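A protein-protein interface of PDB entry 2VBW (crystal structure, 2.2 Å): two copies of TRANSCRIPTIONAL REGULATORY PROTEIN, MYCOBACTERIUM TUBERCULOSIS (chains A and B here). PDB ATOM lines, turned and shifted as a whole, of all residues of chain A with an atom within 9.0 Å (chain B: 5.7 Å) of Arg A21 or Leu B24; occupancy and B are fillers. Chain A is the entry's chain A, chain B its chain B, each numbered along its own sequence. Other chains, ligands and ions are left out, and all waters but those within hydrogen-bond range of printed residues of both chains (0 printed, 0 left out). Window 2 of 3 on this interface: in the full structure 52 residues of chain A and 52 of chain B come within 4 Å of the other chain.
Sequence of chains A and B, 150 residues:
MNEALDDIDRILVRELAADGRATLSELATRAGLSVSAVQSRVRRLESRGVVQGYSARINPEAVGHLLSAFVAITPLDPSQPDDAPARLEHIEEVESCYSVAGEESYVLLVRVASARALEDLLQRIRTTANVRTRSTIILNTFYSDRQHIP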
ATOM      1  N   GLU A  15      32.764 -16.565  21.384  1.00  0.00           N
ATOM      2  CA  GLU A  15      31.698 -17.532  21.095  1.00  0.00           C
ATOM      3  C   GLU A  15      30.357 -16.847  20.857  1.00  0.00           C
ATOM      4  O   GLU A  15      29.593 -17.237  19.965  1.00  0.00           O
ATOM      5  CB  GLU A  15      31.550 -18.517  22.272  1.00  0.00           C
ATOM      6  CG  GLU A  15      32.723 -19.373  22.511  1.00  0.00           C
ATOM      7  CD  GLU A  15      32.993 -20.272  21.336  1.00  0.00           C
ATOM      8  OE1 GLU A  15      32.016 -20.749  20.701  1.00  0.00           O
ATOM      9  OE2 GLU A  15      34.187 -20.482  21.041  1.00  0.00           O
ATOM     10  N   LEU A  16      30.057 -15.838  21.657  1.00  0.00           N
ATOM     11  CA  LEU A  16      28.791 -15.150  21.536  1.00  0.00           C
ATOM     12  C   LEU A  16      28.707 -14.235  20.300  1.00  0.00           C
ATOM     13  O   LEU A  16      27.626 -14.078  19.755  1.00  0.00           O
ATOM     14  CB  LEU A  16      28.448 -14.393  22.831  1.00  0.00           C
ATOM     15  CG  LEU A  16      27.854 -15.210  24.004  1.00  0.00           C
ATOM     16  CD1 LEU A  16      27.920 -14.417  25.357  1.00  0.00           C
ATOM     17  CD2 LEU A  16      26.421 -15.716  23.732  1.00  0.00           C
ATOM     18  N   ALA A  17      29.827 -13.652  19.852  1.00  0.00           N
ATOM     19  CA  ALA A  17      29.855 -12.973  18.524  1.00  0.00           C
ATOM     20  C   ALA A  17      29.567 -13.918  17.344  1.00  0.00           C
ATOM     21  O   ALA A  17      28.858 -13.540  16.397  1.00  0.00           O
ATOM     22  CB  ALA A  17      31.199 -12.230  18.290  1.00  0.00           C
ATOM     23  N   ALA A  18      30.097 -15.133  17.403  1.00  0.00           N
ATOM     24  CA  ALA A  18      29.876 -16.096  16.337  1.00  0.00           C
ATOM     25  C   ALA A  18      28.506 -16.736  16.455  1.00  0.00           C
ATOM     26  O   ALA A  18      27.858 -17.066  15.429  1.00  0.00           O
ATOM     27  CB  ALA A  18      30.989 -17.155  16.314  1.00  0.00           C
ATOM     28  N   ASP A  19      28.017 -16.901  17.697  1.00  0.00           N
ATOM     29  CA  ASP A  19      26.710 -17.535  17.853  1.00  0.00           C
ATOM     30  C   ASP A  19      25.933 -16.976  19.023  1.00  0.00           C
ATOM     31  O   ASP A  19      26.027 -17.497  20.144  1.00  0.00           O
ATOM     32  CB  ASP A  19      26.913 -19.047  18.029  1.00  0.00           C
ATOM     33  CG  ASP A  19      25.607 -19.791  18.284  1.00  0.00           C
ATOM     34  OD1 ASP A  19      24.473 -19.263  18.008  1.00  0.00           O
ATOM     35  OD2 ASP A  19      25.741 -20.934  18.748  1.00  0.00           O
ATOM     36  N   GLY A  20      25.176 -15.930  18.765  1.00  0.00           N
ATOM     37  CA  GLY A  20      24.481 -15.200  19.792  1.00  0.00           C
ATOM     38  C   GLY A  20      23.346 -15.942  20.476  1.00  0.00           C
ATOM     39  O   GLY A  20      22.845 -15.483  21.464  1.00  0.00           O
ATOM     40  N   ARG A  21      22.942 -17.086  19.947  1.00  0.00           N
ATOM     41  CA  ARG A  21      21.947 -17.939  20.619  1.00  0.00           C
ATOM     42  C   ARG A  21      22.584 -19.147  21.361  1.00  0.00           C
ATOM     43  O   ARG A  21      21.853 -20.009  21.786  1.00  0.00           O
ATOM     44  CB  ARG A  21      20.907 -18.466  19.604  1.00  0.00           C
ATOM     45  CG  ARG A  21      19.823 -17.474  19.259  1.00  0.00           C
ATOM     46  CD  ARG A  21      18.733 -18.050  18.298  1.00  0.00           C
ATOM     47  NE  ARG A  21      17.633 -18.717  19.002  1.00  0.00           N
ATOM     48  CZ  ARG A  21      16.727 -18.098  19.764  1.00  0.00           C
ATOM     49  NH1 ARG A  21      16.774 -16.787  19.936  1.00  0.00           N
ATOM     50  NH2 ARG A  21      15.753 -18.795  20.365  1.00  0.00           N
ATOM     51  N   ALA A  22      23.915 -19.199  21.475  1.00  0.00           N
ATOM     52  CA  ALA A  22      24.658 -20.283  22.154  1.00  0.00           C
ATOM     53  C   ALA A  22      24.088 -20.494  23.554  1.00  0.00           C
ATOM     54  O   ALA A  22      23.849 -19.520  24.292  1.00  0.00           O
ATOM     55  N   THR A  23      23.817 -21.732  23.952  1.00  0.00           N
ATOM     56  CA  THR A  23      23.266 -21.869  25.324  1.00  0.00           C
ATOM     57  C   THR A  23      24.318 -21.807  26.399  1.00  0.00           C
ATOM     58  O   THR A  23      25.498 -22.124  26.174  1.00  0.00           O
ATOM     59  CB  THR A  23      22.418 -23.100  25.549  1.00  0.00           C
ATOM     60  OG1 THR A  23      22.879 -24.156  24.687  1.00  0.00           O
ATOM     61  CG2 THR A  23      20.887 -22.775  25.334  1.00  0.00           C
ATOM     62  N   LEU A  24      23.880 -21.351  27.561  1.00  0.00           N
ATOM     63  CA  LEU A  24      24.764 -21.215  28.720  1.00  0.00           C
ATOM     64  C   LEU A  24      25.576 -22.516  28.916  1.00  0.00           C
ATOM     65  O   LEU A  24      26.787 -22.502  29.169  1.00  0.00           O
ATOM     66  CB  LEU A  24      23.911 -20.862  29.934  1.00  0.00           C
ATOM     67  CG  LEU A  24      23.697 -19.410  30.379  1.00  0.00           C
ATOM     68  CD1 LEU A  24      24.207 -18.337  29.396  1.00  0.00           C
ATOM     69  CD2 LEU A  24      22.217 -19.171  30.781  1.00  0.00           C
ATOM     70  N   SER A  25      24.933 -23.650  28.712  1.00  0.00           N
ATOM     71  CA  SER A  25      25.629 -24.889  28.901  1.00  0.00           C
ATOM     72  C   SER A  25      26.632 -25.195  27.817  1.00  0.00           C
ATOM     73  O   SER A  25      27.652 -25.790  28.139  1.00  0.00           O
ATOM     74  CB  SER A  25      24.667 -26.068  29.116  1.00  0.00           C
ATOM     75  OG  SER A  25      23.824 -26.205  27.997  1.00  0.00           O
ATOM     76  N   GLU A  26      26.364 -24.830  26.547  1.00  0.00           N
ATOM     77  CA  GLU A  26      27.414 -24.974  25.491  1.00  0.00           C
ATOM     78  C   GLU A  26      28.605 -24.085  25.882  1.00  0.00           C
ATOM     79  O   GLU A  26      29.754 -24.505  25.850  1.00  0.00           O
ATOM     80  CB  GLU A  26      26.964 -24.604  24.059  1.00  0.00           C
ATOM     81  CG  GLU A  26      25.599 -25.066  23.536  1.00  0.00           C
ATOM     82  CD  GLU A  26      25.197 -24.312  22.200  1.00  0.00           C
ATOM     83  OE1 GLU A  26      24.077 -23.713  22.112  1.00  0.00           O
ATOM     84  OE2 GLU A  26      26.035 -24.293  21.237  1.00  0.00           O
ATOM     85  N   LEU A  27      28.314 -22.848  26.287  1.00  0.00           N
ATOM     86  CA  LEU A  27      29.375 -21.901  26.690  1.00  0.00           C
ATOM     87  C   LEU A  27      30.220 -22.373  27.904  1.00  0.00           C
ATOM     88  O   LEU A  27      31.454 -22.208  27.910  1.00  0.00           O
ATOM     89  CB  LEU A  27      28.759 -20.545  26.989  1.00  0.00           C
ATOM     90  CG  LEU A  27      28.136 -19.764  25.819  1.00  0.00           C
ATOM     91  CD1 LEU A  27      27.396 -18.516  26.333  1.00  0.00           C
ATOM     92  CD2 LEU A  27      29.215 -19.380  24.814  1.00  0.00           C
ATOM     93  N   ARG A  30      32.796 -24.997  26.761  1.00  0.00           N
ATOM     94  CA  ARG A  30      33.916 -24.334  26.061  1.00  0.00           C
ATOM     95  C   ARG A  30      34.884 -23.586  26.995  1.00  0.00           C
ATOM     96  O   ARG A  30      36.090 -23.595  26.767  1.00  0.00           O
ATOM     97  CB  ARG A  30      33.410 -23.432  24.915  1.00  0.00           C
ATOM     98  CG  ARG A  30      33.002 -24.227  23.648  1.00  0.00           C
ATOM     99  CD  ARG A  30      32.023 -23.462  22.742  1.00  0.00           C
ATOM    100  NE  ARG A  30      31.083 -24.352  22.044  1.00  0.00           N
ATOM    101  CZ  ARG A  30      29.860 -23.996  21.607  1.00  0.00           C
ATOM    102  NH1 ARG A  30      29.389 -22.748  21.772  1.00  0.00           N
ATOM    103  NH2 ARG A  30      29.078 -24.896  20.997  1.00  0.00           N
ATOM    104  N   TYR A  54      21.876  -8.566  21.357  1.00  0.00           N
ATOM    105  CA  TYR A  54      21.953  -9.771  20.517  1.00  0.00           C
ATOM    106  C   TYR A  54      20.969  -9.551  19.374  1.00  0.00           C
ATOM    107  O   TYR A  54      19.857  -9.064  19.630  1.00  0.00           O
ATOM    108  CB  TYR A  54      21.544 -11.041  21.336  1.00  0.00           C
ATOM    109  CG  TYR A  54      22.301 -11.219  22.640  1.00  0.00           C
ATOM    110  CD1 TYR A  54      21.864 -10.634  23.815  1.00  0.00           C
ATOM    111  CD2 TYR A  54      23.471 -11.954  22.682  1.00  0.00           C
ATOM    112  CE1 TYR A  54      22.610 -10.777  25.030  1.00  0.00           C
ATOM    113  CE2 TYR A  54      24.205 -12.103  23.867  1.00  0.00           C
ATOM    114  CZ  TYR A  54      23.762 -11.523  25.030  1.00  0.00           C
ATOM    115  OH  TYR A  54      24.507 -11.689  26.185  1.00  0.00           O
ATOM    116  N   SER A  55      21.331  -9.896  18.142  1.00  0.00           N
ATOM    117  CA  SER A  55      20.388  -9.758  17.016  1.00  0.00           C
ATOM    118  C   SER A  55      20.504 -10.924  16.113  1.00  0.00           C
ATOM    119  O   SER A  55      21.602 -11.420  15.942  1.00  0.00           O
ATOM    120  CB  SER A  55      20.739  -8.537  16.132  1.00  0.00           C
ATOM    121  OG  SER A  55      20.936  -7.405  16.922  1.00  0.00           O
ATOM    122  N   ALA A  56      19.386 -11.329  15.512  1.00  0.00           N
ATOM    123  CA  ALA A  56      19.439 -12.111  14.294  1.00  0.00           C
ATOM    124  C   ALA A  56      20.013 -11.205  13.171  1.00  0.00           C
ATOM    125  O   ALA A  56      19.706 -10.024  13.118  1.00  0.00           O
ATOM    126  CB  ALA A  56      18.032 -12.626  13.917  1.00  0.00           C
ATOM    127  N   ARG A  57      20.858 -11.768  12.325  1.00  0.00           N
ATOM    128  CA  ARG A  57      21.327 -11.113  11.096  1.00  0.00           C
ATOM    129  C   ARG A  57      20.327 -11.370   9.962  1.00  0.00           C
ATOM    130  O   ARG A  57      20.265 -12.487   9.434  1.00  0.00           O
ATOM    131  CB  ARG A  57      22.667 -11.647  10.701  1.00  0.00           C
ATOM    132  N   LEU B  16      13.255 -10.968  16.508  1.00  0.00           N
ATOM    133  CA  LEU B  16      14.570 -11.593  16.582  1.00  0.00           C
ATOM    134  C   LEU B  16      15.722 -10.655  16.193  1.00  0.00           C
ATOM    135  O   LEU B  16      16.852 -10.846  16.664  1.00  0.00           O
ATOM    136  CB  LEU B  16      14.625 -12.844  15.692  1.00  0.00           C
ATOM    137  CG  LEU B  16      14.162 -14.240  16.191  1.00  0.00           C
ATOM    138  CD1 LEU B  16      14.147 -15.213  15.017  1.00  0.00           C
ATOM    139  CD2 LEU B  16      15.024 -14.803  17.349  1.00  0.00           C
ATOM    140  N   ASP B  19      15.861  -8.684  19.457  1.00  0.00           N
ATOM    141  CA  ASP B  19      16.402  -9.516  20.568  1.00  0.00           C
ATOM    142  C   ASP B  19      16.665 -10.932  20.083  1.00  0.00           C
ATOM    143  O   ASP B  19      15.778 -11.762  20.127  1.00  0.00           O
ATOM    144  CB  ASP B  19      15.425  -9.567  21.767  1.00  0.00           C
ATOM    145  CG  ASP B  19      16.025 -10.270  23.034  1.00  0.00           C
ATOM    146  OD1 ASP B  19      17.186 -10.808  23.035  1.00  0.00           O
ATOM    147  OD2 ASP B  19      15.304 -10.259  24.062  1.00  0.00           O
ATOM    148  N   GLY B  20      17.888 -11.196  19.654  1.00  0.00           N
ATOM    149  CA  GLY B  20      18.250 -12.446  19.008  1.00  0.00           C
ATOM    150  C   GLY B  20      18.366 -13.614  19.968  1.00  0.00           C
ATOM    151  O   GLY B  20      18.530 -14.742  19.530  1.00  0.00           O
ATOM    152  N   ARG B  21      18.284 -13.327  21.268  1.00  0.00           N
ATOM    153  CA  ARG B  21      18.153 -14.345  22.313  1.00  0.00           C
ATOM    154  C   ARG B  21      16.717 -14.527  22.840  1.00  0.00           C
ATOM    155  O   ARG B  21      16.528 -15.173  23.867  1.00  0.00           O
ATOM    156  CB  ARG B  21      19.093 -14.060  23.498  1.00  0.00           C
ATOM    157  CG  ARG B  21      20.460 -14.613  23.300  1.00  0.00           C
ATOM    158  CD  ARG B  21      21.357 -14.413  24.504  1.00  0.00           C
ATOM    159  NE  ARG B  21      21.424 -15.635  25.308  1.00  0.00           N
ATOM    160  CZ  ARG B  21      22.187 -16.694  25.033  1.00  0.00           C
ATOM    161  NH1 ARG B  21      22.980 -16.708  23.964  1.00  0.00           N
ATOM    162  NH2 ARG B  21      22.176 -17.760  25.847  1.00  0.00           N
ATOM    163  N   ALA B  22      15.719 -13.952  22.165  1.00  0.00           N
ATOM    164  CA  ALA B  22      14.309 -14.225  22.479  1.00  0.00           C
ATOM    165  C   ALA B  22      14.100 -15.738  22.517  1.00  0.00           C
ATOM    166  O   ALA B  22      14.705 -16.490  21.725  1.00  0.00           O
ATOM    167  N   THR B  23      13.294 -16.206  23.468  1.00  0.00           N
ATOM    168  CA  THR B  23      12.990 -17.654  23.503  1.00  0.00           C
ATOM    169  C   THR B  23      11.741 -17.981  22.721  1.00  0.00           C
ATOM    170  O   THR B  23      10.823 -17.169  22.633  1.00  0.00           O
ATOM    171  CB  THR B  23      12.976 -18.306  24.927  1.00  0.00           C
ATOM    172  OG1 THR B  23      12.780 -17.305  25.942  1.00  0.00           O
ATOM    173  CG2 THR B  23      14.297 -19.084  25.185  1.00  0.00           C
ATOM    174  N   LEU B  24      11.740 -19.175  22.134  1.00  0.00           N
ATOM    175  CA  LEU B  24      10.690 -19.637  21.227  1.00  0.00           C
ATOM    176  C   LEU B  24       9.312 -19.631  21.900  1.00  0.00           C
ATOM    177  O   LEU B  24       8.277 -19.707  21.226  1.00  0.00           O
ATOM    178  CB  LEU B  24      11.048 -21.024  20.672  1.00  0.00           C
ATOM    179  CG  LEU B  24      12.512 -21.204  20.223  1.00  0.00           C
ATOM    180  CD1 LEU B  24      13.500 -21.376  21.426  1.00  0.00           C
ATOM    181  CD2 LEU B  24      12.665 -22.364  19.216  1.00  0.00           C
ATOM    182  N   SER B  25       9.320 -19.506  23.227  1.00  0.00           N
ATOM    183  CA  SER B  25       8.107 -19.470  24.041  1.00  0.00           C
ATOM    184  C   SER B  25       7.691 -18.043  24.423  1.00  0.00           C
ATOM    185  O   SER B  25       6.497 -17.731  24.424  1.00  0.00           O
ATOM    186  CB  SER B  25       8.264 -20.349  25.297  1.00  0.00           C
ATOM    187  OG  SER B  25       9.182 -19.780  26.227  1.00  0.00           O
ATOM    188  N   GLU B  26       8.664 -17.192  24.765  1.00  0.00           N
ATOM    189  CA  GLU B  26       8.416 -15.752  24.965  1.00  0.00           C
ATOM    190  C   GLU B  26       8.115 -15.082  23.616  1.00  0.00           C
ATOM    191  O   GLU B  26       7.609 -13.958  23.580  1.00  0.00           O
ATOM    192  CB  GLU B  26       9.594 -15.065  25.679  1.00  0.00           C
ATOM    193  N   LEU B  27       8.416 -15.790  22.521  1.00  0.00           N
ATOM    194  CA  LEU B  27       8.062 -15.351  21.163  1.00  0.00           C
ATOM    195  C   LEU B  27       6.603 -15.640  20.864  1.00  0.00           C
ATOM    196  O   LEU B  27       5.845 -14.722  20.554  1.00  0.00           O
ATOM    197  CB  LEU B  27       8.952 -16.011  20.084  1.00  0.00           C
ATOM    198  CG  LEU B  27      10.319 -15.423  19.672  1.00  0.00           C
ATOM    199  CD1 LEU B  27      10.917 -16.226  18.519  1.00  0.00           C
ATOM    200  CD2 LEU B  27      10.247 -13.939  19.310  1.00  0.00           C
ATOM    201  N   ALA B  28       6.231 -16.920  20.969  1.00  0.00           N
ATOM    202  CA  ALA B  28       4.872 -17.428  20.702  1.00  0.00           C
ATOM    203  C   ALA B  28       3.748 -16.573  21.276  1.00  0.00           C
ATOM    204  O   ALA B  28       2.744 -16.353  20.597  1.00  0.00           O
ATOM    205  CB  ALA B  28       4.739 -18.872  21.179  1.00  0.00           C
ATOM    206  N   VAL B  35       4.625 -22.919  20.157  1.00  0.00           N
ATOM    207  CA  VAL B  35       6.034 -23.372  20.075  1.00  0.00           C
ATOM    208  C   VAL B  35       6.411 -24.228  18.832  1.00  0.00           C
ATOM    209  O   VAL B  35       7.499 -24.062  18.268  1.00  0.00           O
ATOM    210  CB  VAL B  35       6.509 -24.058  21.427  1.00  0.00           C
ATOM    211  CG1 VAL B  35       7.813 -24.881  21.253  1.00  0.00           C
ATOM    212  CG2 VAL B  35       6.675 -23.020  22.560  1.00  0.00           C
ATOM    213  N   VAL B  38       6.099 -21.683  15.715  1.00  0.00           N
ATOM    214  CA  VAL B  38       7.211 -20.751  15.957  1.00  0.00           C
ATOM    215  C   VAL B  38       8.550 -21.396  15.598  1.00  0.00           C
ATOM    216  O   VAL B  38       9.290 -20.865  14.779  1.00  0.00           O
ATOM    217  CB  VAL B  38       7.216 -20.218  17.426  1.00  0.00           C
ATOM    218  CG1 VAL B  38       8.467 -19.417  17.723  1.00  0.00           C
ATOM    219  CG2 VAL B  38       5.995 -19.360  17.691  1.00  0.00           C
ATOM    220  N   GLN B  39       8.831 -22.555  16.176  1.00  0.00           N
ATOM    221  CA  GLN B  39      10.074 -23.269  15.905  1.00  0.00           C
ATOM    222  C   GLN B  39      10.279 -23.674  14.445  1.00  0.00           C
ATOM    223  O   GLN B  39      11.417 -23.728  13.953  1.00  0.00           O
ATOM    224  CB  GLN B  39      10.153 -24.519  16.773  1.00  0.00           C
ATOM    225  CG  GLN B  39      11.417 -25.340  16.584  1.00  0.00           C
ATOM    226  CD  GLN B  39      11.492 -26.500  17.551  1.00  0.00           C
ATOM    227  OE1 GLN B  39      11.682 -27.656  17.140  1.00  0.00           O
ATOM    228  NE2 GLN B  39      11.333 -26.207  18.851  1.00  0.00           N
ATOM    229  N   TYR B  54      22.991 -15.341  14.237  1.00  0.00           N
ATOM    230  CA  TYR B  54      22.641 -14.579  15.434  1.00  0.00           C
ATOM    231  C   TYR B  54      23.958 -14.138  15.993  1.00  0.00           C
ATOM    232  O   TYR B  54      24.931 -14.891  15.933  1.00  0.00           O
ATOM    233  CB  TYR B  54      21.899 -15.456  16.444  1.00  0.00           C
ATOM    234  CG  TYR B  54      20.624 -16.026  15.878  1.00  0.00           C
ATOM    235  CD1 TYR B  54      20.641 -17.221  15.168  1.00  0.00           C
ATOM    236  CD2 TYR B  54      19.409 -15.372  16.087  1.00  0.00           C
ATOM    237  CE1 TYR B  54      19.477 -17.745  14.629  1.00  0.00           C
ATOM    238  CE2 TYR B  54      18.227 -15.874  15.596  1.00  0.00           C
ATOM    239  CZ  TYR B  54      18.261 -17.062  14.854  1.00  0.00           C
ATOM    240  OH  TYR B  54      17.087 -17.574  14.349  1.00  0.00           O
ATOM    241  N   SER B  55      24.039 -12.906  16.479  1.00  0.00           N
ATOM    242  CA  SER B  55      25.312 -12.492  17.036  1.00  0.00           C
ATOM    243  C   SER B  55      25.113 -11.617  18.265  1.00  0.00           C
ATOM    244  O   SER B  55      24.098 -10.930  18.404  1.00  0.00           O
ATOM    245  CB  SER B  55      26.282 -11.791  15.899  1.00  0.00           C
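Arg A21 touches six residues of chain B.
Leu B24 touches just one residue of chain A: Arg A21 (3.6 Å).
Ala B22 touches just one residue of chain A: Arg A21 (2.8 Å).
No residue of chain A comes within 4 Å of Thr B23.
Ser B25 touches none of the printed residues of chain A.
Of the printed residues of chain A, Asp B19 touches Tyr A54 (3.6 Å).
Of the printed residues of chain A, Leu B16 touches Arg A21 (3.7 Å), Ser A55 (3.7 Å) and Ala A56 (2.8 Å).
Printed residues of chain B within 4 Å of Ala A22: Arg B21 (2.9 Å).
Of the printed residues of chain A, Tyr B54 touches Ala A18, Asp A19, Gly A20, Arg A21, Ser A55 and Ala A56.
Of the printed residues of chain B, Ala A18 touches Tyr B54.
Glu A15 touches none of the printed residues of chain B.
The nearest residue of chain A that does not touch Leu B24 is Thr A23 (8.5 Å).
Printed residues of chain B that touch a printed residue of chain A: Leu B16, Asp B19, Gly B20, Arg B21, Ala B22, Leu B24, Tyr B54 and Ser B55.
Hydrophobic or aromatic side chains of chain B that line the printed part of chain A: Leu B16, Leu B24 and Tyr B54.
Along chain B the printed residues that touch a printed residue of chain A span positions 16 to 55.
Hydrophobic or aromatic side chains of chain A that line the printed part of chain B: Leu A16, Tyr A54 and Ala A56.
Among the printed residues, 26 pairs touch across the chains.
Among the printed residues, no Asp or Glu carboxylate lies within 4 Å of a Lys or Arg side-chain nitrogen of the other chain.
Arg B21 touches Leu A16 (NH1 to CD2, 3.6 Å).
Leu A16 touches Ser B55.
Ser B55 touches Ala A17 (CB to O, 3.2 Å).
O of Ala A18 touches O of Tyr B54, 3.7 Å away.
Arg A21 touches Leu B16.
Leu B24 touches Arg A21.
Arg A21 touches Tyr B54.
O of Tyr A54 touches CA of Asp B19 (3.6 Å).
Tyr A54 touches Ser B55.
C of Ser A55 touches O of Leu B16, 3.7 Å away.
The side-chain carboxylate of Asp A19 lies close to the backbone NH of Arg A21, 3.3 Å away.
OD1 of Asp B19 lies close to N of Arg B21, 3.3 Å away.
Leu A16 touches Ser B55, and with the chains exchanged Ser A55 touches Leu B16.
Gly A20 touches Arg B21, and with the chains exchanged Arg A21 touches Gly B20.
Arg A21 touches Ala B22, and with the chains exchanged Ala A22 touches Arg B21.
Arg A21 touches Tyr B54, and with the chains exchanged Tyr A54 touches Arg B21.
Positions printed for both chains: 16, 19, 20, 21, 22, 23, 24, 25, 26, 27, 54 and 55.
NH1 of Arg B21 lies within hydrogen-bond range of O of Gly A20 (2.8 Å).
The backbone NH (N) of Gly A20 sits at hydrogen-bond distance from the backbone carbonyl oxygen (O) of Tyr B54 (3.0 Å).
The guanidinium group of Arg A21 sits at hydrogen-bond distance from the backbone carbonyl oxygen of Gly B20.
The guanidinium group (NH1) of Arg A21 sits at hydrogen-bond distance from the backbone carbonyl oxygen (O) of Ala B22 (2.8 Å).
The guanidinium group (NH2) of Arg B21 is in hydrogen-bond range of the backbone carbonyl oxygen (O) of Ala A22 (2.9 Å).
O of Tyr A54 is in hydrogen-bond range of N of Gly B20 (2.9 Å).
O of Ser A55 lies within hydrogen-bond range of N of Ser B55.
N of Ala A56 sits at hydrogen-bond distance from O of Leu B16 (2.8 Å).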
